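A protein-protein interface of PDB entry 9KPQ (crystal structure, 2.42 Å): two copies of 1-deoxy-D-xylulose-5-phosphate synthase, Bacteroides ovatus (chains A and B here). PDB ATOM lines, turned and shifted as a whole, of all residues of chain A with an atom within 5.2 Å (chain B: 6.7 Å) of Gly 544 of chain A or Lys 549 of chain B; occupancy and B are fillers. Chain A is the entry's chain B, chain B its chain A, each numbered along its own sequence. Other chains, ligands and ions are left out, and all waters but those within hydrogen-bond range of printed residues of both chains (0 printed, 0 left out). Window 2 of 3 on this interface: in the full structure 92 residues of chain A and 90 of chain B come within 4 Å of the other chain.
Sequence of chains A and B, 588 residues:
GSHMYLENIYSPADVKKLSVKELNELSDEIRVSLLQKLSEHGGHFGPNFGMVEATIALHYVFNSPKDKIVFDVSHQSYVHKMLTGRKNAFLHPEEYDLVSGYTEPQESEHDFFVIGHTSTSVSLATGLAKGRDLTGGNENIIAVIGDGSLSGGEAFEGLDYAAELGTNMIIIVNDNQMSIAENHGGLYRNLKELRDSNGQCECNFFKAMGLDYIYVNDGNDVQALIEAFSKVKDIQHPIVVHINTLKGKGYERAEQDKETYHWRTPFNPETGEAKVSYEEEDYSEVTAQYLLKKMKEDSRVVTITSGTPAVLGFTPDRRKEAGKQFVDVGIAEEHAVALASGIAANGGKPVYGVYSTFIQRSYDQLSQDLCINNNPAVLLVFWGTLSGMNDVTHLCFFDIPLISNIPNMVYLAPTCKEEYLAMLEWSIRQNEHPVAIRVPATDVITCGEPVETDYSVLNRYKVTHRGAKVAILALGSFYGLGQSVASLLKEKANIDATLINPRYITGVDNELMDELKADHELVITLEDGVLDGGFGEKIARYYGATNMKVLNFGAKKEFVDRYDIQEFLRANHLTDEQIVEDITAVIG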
ATOM      1  N   ALA A 540      19.663  17.396  13.938  1.00  0.00           N
ATOM      2  CA  ALA A 540      19.247  17.619  12.561  1.00  0.00           C
ATOM      3  C   ALA A 540      20.122  16.822  11.607  1.00  0.00           C
ATOM      4  O   ALA A 540      19.623  16.151  10.697  1.00  0.00           O
ATOM      5  CB  ALA A 540      19.292  19.099  12.214  1.00  0.00           C
ATOM      6  N   ARG A 541      21.428  16.896  11.824  1.00  0.00           N
ATOM      7  CA  ARG A 541      22.383  16.207  10.976  1.00  0.00           C
ATOM      8  C   ARG A 541      22.149  14.702  11.010  1.00  0.00           C
ATOM      9  O   ARG A 541      22.222  14.045   9.968  1.00  0.00           O
ATOM     10  CB  ARG A 541      23.816  16.522  11.404  1.00  0.00           C
ATOM     11  CG  ARG A 541      24.849  15.587  10.824  1.00  0.00           C
ATOM     12  CD  ARG A 541      26.216  16.250  10.644  1.00  0.00           C
ATOM     13  NE  ARG A 541      26.867  16.596  11.904  1.00  0.00           N
ATOM     14  CZ  ARG A 541      27.691  15.795  12.568  1.00  0.00           C
ATOM     15  NH1 ARG A 541      27.967  14.575  12.137  1.00  0.00           N
ATOM     16  NH2 ARG A 541      28.262  16.234  13.686  1.00  0.00           N
ATOM     17  N   TYR A 542      21.868  14.168  12.202  1.00  0.00           N
ATOM     18  CA  TYR A 542      21.715  12.733  12.374  1.00  0.00           C
ATOM     19  C   TYR A 542      20.576  12.181  11.515  1.00  0.00           C
ATOM     20  O   TYR A 542      20.679  11.079  10.972  1.00  0.00           O
ATOM     21  CB  TYR A 542      21.455  12.386  13.847  1.00  0.00           C
ATOM     22  CG  TYR A 542      21.437  10.890  14.132  1.00  0.00           C
ATOM     23  CD1 TYR A 542      22.614  10.154  14.170  1.00  0.00           C
ATOM     24  CD2 TYR A 542      20.239  10.211  14.346  1.00  0.00           C
ATOM     25  CE1 TYR A 542      22.605   8.790  14.422  1.00  0.00           C
ATOM     26  CE2 TYR A 542      20.221   8.837  14.599  1.00  0.00           C
ATOM     27  CZ  TYR A 542      21.409   8.130  14.632  1.00  0.00           C
ATOM     28  OH  TYR A 542      21.415   6.768  14.883  1.00  0.00           O
ATOM     29  N   TYR A 543      19.498  12.956  11.403  1.00  0.00           N
ATOM     30  CA  TYR A 543      18.270  12.531  10.729  1.00  0.00           C
ATOM     31  C   TYR A 543      18.235  12.975   9.276  1.00  0.00           C
ATOM     32  O   TYR A 543      17.236  12.785   8.586  1.00  0.00           O
ATOM     33  CB  TYR A 543      17.037  13.097  11.441  1.00  0.00           C
ATOM     34  CG  TYR A 543      16.600  12.360  12.681  1.00  0.00           C
ATOM     35  CD1 TYR A 543      16.360  10.980  12.667  1.00  0.00           C
ATOM     36  CD2 TYR A 543      16.396  13.047  13.864  1.00  0.00           C
ATOM     37  CE1 TYR A 543      15.940  10.310  13.822  1.00  0.00           C
ATOM     38  CE2 TYR A 543      15.976  12.392  15.013  1.00  0.00           C
ATOM     39  CZ  TYR A 543      15.751  11.029  14.989  1.00  0.00           C
ATOM     40  OH  TYR A 543      15.348  10.419  16.151  1.00  0.00           O
ATOM     41  N   GLY A 544      19.335  13.558   8.815  1.00  0.00           N
ATOM     42  CA  GLY A 544      19.379  14.172   7.501  1.00  0.00           C
ATOM     43  C   GLY A 544      19.027  13.284   6.318  1.00  0.00           C
ATOM     44  O   GLY A 544      18.543  13.781   5.293  1.00  0.00           O
ATOM     45  N   ALA A 545      19.274  11.982   6.456  1.00  0.00           N
ATOM     46  CA  ALA A 545      19.025  11.024   5.381  1.00  0.00           C
ATOM     47  C   ALA A 545      17.838  10.120   5.695  1.00  0.00           C
ATOM     48  O   ALA A 545      17.537   9.185   4.951  1.00  0.00           O
ATOM     49  CB  ALA A 545      20.269  10.187   5.119  1.00  0.00           C
ATOM     50  N   THR A 546      17.182  10.384   6.814  1.00  0.00           N
ATOM     51  CA  THR A 546      16.025   9.608   7.233  1.00  0.00           C
ATOM     52  C   THR A 546      14.753  10.377   6.891  1.00  0.00           C
ATOM     53  O   THR A 546      14.827  11.480   6.358  1.00  0.00           O
ATOM     54  CB  THR A 546      16.057   9.321   8.727  1.00  0.00           C
ATOM     55  OG1 THR A 546      15.617  10.492   9.429  1.00  0.00           O
ATOM     56  CG2 THR A 546      17.467   8.963   9.161  1.00  0.00           C
ATOM     57  N   ASN A 547      13.592   9.793   7.175  1.00  0.00           N
ATOM     58  CA  ASN A 547      12.328  10.464   6.883  1.00  0.00           C
ATOM     59  C   ASN A 547      11.786  11.207   8.101  1.00  0.00           C
ATOM     60  O   ASN A 547      10.653  11.696   8.084  1.00  0.00           O
ATOM     61  CB  ASN A 547      11.296   9.468   6.361  1.00  0.00           C
ATOM     62  CG  ASN A 547      11.544   9.102   4.914  1.00  0.00           C
ATOM     63  OD1 ASN A 547      11.965   9.940   4.118  1.00  0.00           O
ATOM     64  ND2 ASN A 547      11.270   7.857   4.562  1.00  0.00           N
ATOM     65  N   HIS B 520      15.362  18.461  -7.090  1.00  0.00           N
ATOM     66  CA  HIS B 520      16.374  17.750  -6.312  1.00  0.00           C
ATOM     67  C   HIS B 520      15.723  17.150  -5.083  1.00  0.00           C
ATOM     68  O   HIS B 520      14.770  17.714  -4.534  1.00  0.00           O
ATOM     69  CB  HIS B 520      17.522  18.675  -5.882  1.00  0.00           C
ATOM     70  CG  HIS B 520      18.211  19.373  -7.013  1.00  0.00           C
ATOM     71  ND1 HIS B 520      17.766  20.572  -7.527  1.00  0.00           N
ATOM     72  CD2 HIS B 520      19.337  19.063  -7.702  1.00  0.00           C
ATOM     73  CE1 HIS B 520      18.575  20.961  -8.498  1.00  0.00           C
ATOM     74  NE2 HIS B 520      19.541  20.067  -8.620  1.00  0.00           N
ATOM     75  N   GLU B 521      16.242  16.009  -4.645  1.00  0.00           N
ATOM     76  CA  GLU B 521      15.729  15.368  -3.439  1.00  0.00           C
ATOM     77  C   GLU B 521      16.834  15.186  -2.403  1.00  0.00           C
ATOM     78  O   GLU B 521      16.568  14.904  -1.236  1.00  0.00           O
ATOM     79  CB  GLU B 521      15.099  14.020  -3.779  1.00  0.00           C
ATOM     80  CG  GLU B 521      16.122  12.964  -4.084  1.00  0.00           C
ATOM     81  CD  GLU B 521      15.572  11.861  -4.967  1.00  0.00           C
ATOM     82  OE1 GLU B 521      15.429  12.076  -6.193  1.00  0.00           O
ATOM     83  OE2 GLU B 521      15.281  10.774  -4.431  1.00  0.00           O
ATOM     84  N   LEU B 522      18.076  15.340  -2.840  1.00  0.00           N
ATOM     85  CA  LEU B 522      19.213  15.188  -1.949  1.00  0.00           C
ATOM     86  C   LEU B 522      20.210  16.313  -2.136  1.00  0.00           C
ATOM     87  O   LEU B 522      20.624  16.611  -3.270  1.00  0.00           O
ATOM     88  CB  LEU B 522      19.920  13.851  -2.182  1.00  0.00           C
ATOM     89  CG  LEU B 522      21.243  13.696  -1.423  1.00  0.00           C
ATOM     90  CD1 LEU B 522      21.002  13.550   0.100  1.00  0.00           C
ATOM     91  CD2 LEU B 522      22.045  12.531  -1.965  1.00  0.00           C
ATOM     92  N   VAL B 523      20.615  16.921  -1.024  1.00  0.00           N
ATOM     93  CA  VAL B 523      21.713  17.879  -1.037  1.00  0.00           C
ATOM     94  C   VAL B 523      22.831  17.355  -0.141  1.00  0.00           C
ATOM     95  O   VAL B 523      22.575  16.864   0.964  1.00  0.00           O
ATOM     96  CB  VAL B 523      21.257  19.279  -0.595  1.00  0.00           C
ATOM     97  CG1 VAL B 523      22.406  20.301  -0.757  1.00  0.00           C
ATOM     98  CG2 VAL B 523      20.059  19.707  -1.409  1.00  0.00           C
ATOM     99  N   ILE B 524      24.063  17.425  -0.638  1.00  0.00           N
ATOM    100  CA  ILE B 524      25.211  17.059   0.175  1.00  0.00           C
ATOM    101  C   ILE B 524      26.200  18.213   0.272  1.00  0.00           C
ATOM    102  O   ILE B 524      26.299  19.055  -0.627  1.00  0.00           O
ATOM    103  CB  ILE B 524      25.916  15.772  -0.353  1.00  0.00           C
ATOM    104  CG1 ILE B 524      26.734  16.055  -1.613  1.00  0.00           C
ATOM    105  CG2 ILE B 524      24.907  14.656  -0.579  1.00  0.00           C
ATOM    106  CD1 ILE B 524      27.785  14.975  -1.893  1.00  0.00           C
ATOM    107  N   ALA B 540      21.722  21.019   7.093  1.00  0.00           N
ATOM    108  CA  ALA B 540      20.855  20.018   7.682  1.00  0.00           C
ATOM    109  C   ALA B 540      19.745  20.718   8.445  1.00  0.00           C
ATOM    110  O   ALA B 540      18.578  20.360   8.303  1.00  0.00           O
ATOM    111  CB  ALA B 540      21.631  19.090   8.587  1.00  0.00           C
ATOM    112  N   TYR B 543      16.897  22.382   6.201  1.00  0.00           N
ATOM    113  CA  TYR B 543      16.004  21.447   5.525  1.00  0.00           C
ATOM    114  C   TYR B 543      15.293  20.514   6.501  1.00  0.00           C
ATOM    115  O   TYR B 543      14.587  19.593   6.085  1.00  0.00           O
ATOM    116  CB  TYR B 543      16.790  20.614   4.527  1.00  0.00           C
ATOM    117  CG  TYR B 543      17.149  21.305   3.235  1.00  0.00           C
ATOM    118  CD1 TYR B 543      16.160  21.767   2.357  1.00  0.00           C
ATOM    119  CD2 TYR B 543      18.479  21.458   2.868  1.00  0.00           C
ATOM    120  CE1 TYR B 543      16.501  22.368   1.157  1.00  0.00           C
ATOM    121  CE2 TYR B 543      18.826  22.065   1.678  1.00  0.00           C
ATOM    122  CZ  TYR B 543      17.837  22.514   0.828  1.00  0.00           C
ATOM    123  OH  TYR B 543      18.212  23.102  -0.354  1.00  0.00           O
ATOM    124  N   THR B 546      11.660  19.950   6.055  1.00  0.00           N
ATOM    125  CA  THR B 546      11.283  19.781   4.656  1.00  0.00           C
ATOM    126  C   THR B 546      11.507  18.345   4.178  1.00  0.00           C
ATOM    127  O   THR B 546      11.989  17.500   4.926  1.00  0.00           O
ATOM    128  CB  THR B 546      12.065  20.751   3.749  1.00  0.00           C
ATOM    129  OG1 THR B 546      13.311  20.154   3.365  1.00  0.00           O
ATOM    130  CG2 THR B 546      12.342  22.047   4.489  1.00  0.00           C
ATOM    131  N   ASN B 547      11.151  18.066   2.928  1.00  0.00           N
ATOM    132  CA  ASN B 547      11.309  16.715   2.410  1.00  0.00           C
ATOM    133  C   ASN B 547      12.629  16.551   1.678  1.00  0.00           C
ATOM    134  O   ASN B 547      12.885  15.510   1.072  1.00  0.00           O
ATOM    135  CB  ASN B 547      10.140  16.351   1.493  1.00  0.00           C
ATOM    136  CG  ASN B 547       8.847  16.163   2.258  1.00  0.00           C
ATOM    137  OD1 ASN B 547       8.015  17.069   2.334  1.00  0.00           O
ATOM    138  ND2 ASN B 547       8.683  14.987   2.855  1.00  0.00           N
ATOM    139  N   MET B 548      13.468  17.581   1.735  1.00  0.00           N
ATOM    140  CA  MET B 548      14.820  17.484   1.185  1.00  0.00           C
ATOM    141  C   MET B 548      15.699  16.646   2.108  1.00  0.00           C
ATOM    142  O   MET B 548      15.737  16.881   3.317  1.00  0.00           O
ATOM    143  CB  MET B 548      15.431  18.868   1.002  1.00  0.00           C
ATOM    144  CG  MET B 548      16.722  18.874   0.230  1.00  0.00           C
ATOM    145  SD  MET B 548      16.380  18.488  -1.499  1.00  0.00           S
ATOM    146  CE  MET B 548      16.544  20.100  -2.271  1.00  0.00           C
ATOM    147  N   LYS B 549      16.405  15.675   1.549  1.00  0.00           N
ATOM    148  CA  LYS B 549      17.360  14.917   2.344  1.00  0.00           C
ATOM    149  C   LYS B 549      18.755  15.514   2.227  1.00  0.00           C
ATOM    150  O   LYS B 549      19.101  16.120   1.200  1.00  0.00           O
ATOM    151  CB  LYS B 549      17.361  13.451   1.930  1.00  0.00           C
ATOM    152  CG  LYS B 549      16.294  12.664   2.648  1.00  0.00           C
ATOM    153  CD  LYS B 549      16.092  11.312   2.031  1.00  0.00           C
ATOM    154  CE  LYS B 549      14.778  10.728   2.513  1.00  0.00           C
ATOM    155  NZ  LYS B 549      14.919   9.279   2.804  1.00  0.00           N
ATOM    156  N   VAL B 550      19.536  15.365   3.299  1.00  0.00           N
ATOM    157  CA  VAL B 550      20.870  15.962   3.391  1.00  0.00           C
ATOM    158  C   VAL B 550      21.888  14.971   3.951  1.00  0.00           C
ATOM    159  O   VAL B 550      21.611  14.269   4.921  1.00  0.00           O
ATOM    160  CB  VAL B 550      20.853  17.237   4.271  1.00  0.00           C
ATOM    161  CG1 VAL B 550      22.283  17.758   4.522  1.00  0.00           C
ATOM    162  CG2 VAL B 550      19.963  18.327   3.662  1.00  0.00           C
ATOM    163  N   LEU B 551      23.061  14.926   3.330  1.00  0.00           N
ATOM    164  CA  LEU B 551      24.226  14.262   3.895  1.00  0.00           C
ATOM    165  C   LEU B 551      25.326  15.295   4.144  1.00  0.00           C
ATOM    166  O   LEU B 551      25.551  16.190   3.312  1.00  0.00           O
ATOM    167  CB  LEU B 551      24.761  13.178   2.960  1.00  0.00           C
ATOM    168  CG  LEU B 551      23.970  11.890   2.776  1.00  0.00           C
ATOM    169  CD1 LEU B 551      24.603  11.116   1.630  1.00  0.00           C
ATOM    170  CD2 LEU B 551      23.912  11.048   4.069  1.00  0.00           C
ATOM    171  N   VAL B 586      21.253   6.197  -0.483  1.00  0.00           N
ATOM    172  CA  VAL B 586      20.164   7.014   0.048  1.00  0.00           C
ATOM    173  C   VAL B 586      19.056   7.152  -0.991  1.00  0.00           C
ATOM    174  O   VAL B 586      17.865   7.110  -0.665  1.00  0.00           O
ATOM    175  CB  VAL B 586      20.671   8.408   0.493  1.00  0.00           C
ATOM    176  CG1 VAL B 586      19.495   9.327   0.830  1.00  0.00           C
ATOM    177  CG2 VAL B 586      21.625   8.280   1.680  1.00  0.00           C
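The backbone NH (N) of Val 550 of chain B sits at hydrogen-bond distance from the backbone carbonyl oxygen (O) of Gly 544 of chain A, 2.7 Å away. The side-chain amino group (NZ) of Lys 549 of chain B is in hydrogen-bond range of the backbone carbonyl oxygen (O) of Ala 545 of chain A. The side-chain amino group (NZ) of Lys 549 of chain B sits at hydrogen-bond distance from the side-chain amide oxygen (OD1) of Asn 547 of chain A, 3.3 Å away.
The backbone carbonyl oxygen (O) of Tyr 543 of chain A is in hydrogen-bond range of the side-chain hydroxyl (OG1) of Thr 546 of chain A. N of Val 523 of chain B sits at hydrogen-bond distance from O of Lys 549 of chain B (2.8 Å). The backbone carbonyl oxygen (O) of Val 523 of chain B is in hydrogen-bond range of the backbone NH (N) of Leu 551 of chain B (3.1 Å). The backbone carbonyl oxygen (O) of Glu 521 of chain B is in hydrogen-bond range of the backbone NH (N) of Lys 549 of chain B (2.9 Å).
CB of Ala 540 of chain B touches CA of Arg 541 of chain A, 3.8 Å away. Gly 544 of chain A touches Lys 549 of chain B. Val 550 of chain B touches Ala 545 of chain A. CB of Ala 545 of chain A touches CD2 of Leu 551 of chain B (3.9 Å). CE of Lys 549 of chain B touches O of Thr 546 of chain A, 3.9 Å away.
Of the printed residues of chain B, Arg 541 of chain A touches Ala 540. Gly 544 of chain A touches just these residues of chain B: Lys 549 and Val 550. Printed residues of chain B within 4 Å of Thr 546 of chain A: Lys 549 (3.9 Å). Asn 547 of chain B touches none of the printed residues of chain A. Printed residues of chain A within 4 Å of Val 550 of chain B: Gly 544 and Ala 545. The nearest printed residue of chain A that does not touch Lys 549 of chain B is Tyr 543 of chain A (6.0 Å). The nearest printed residue of chain A that does not touch Val 550 of chain B is Arg 541 of chain A (5.1 Å).
Hydrophobic or aromatic side chains of chain A within 4 Å of the printed part of chain B: Ala 545. Hydrophobic or aromatic side chains of chain B that line the printed part of chain A: Ala 540 and Leu 551. Among the printed residues, 8 pairs touch across the chains. Among the printed residues, no Asp or Glu carboxylate lies within 4 Å of a Lys or Arg side-chain nitrogen of the other chain.
Positions printed for both chains: 540, 543, 546 and 547. Of the 8 pairs that touch across the chains among the printed residues, none has its exchanged pair printed and touching as well.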
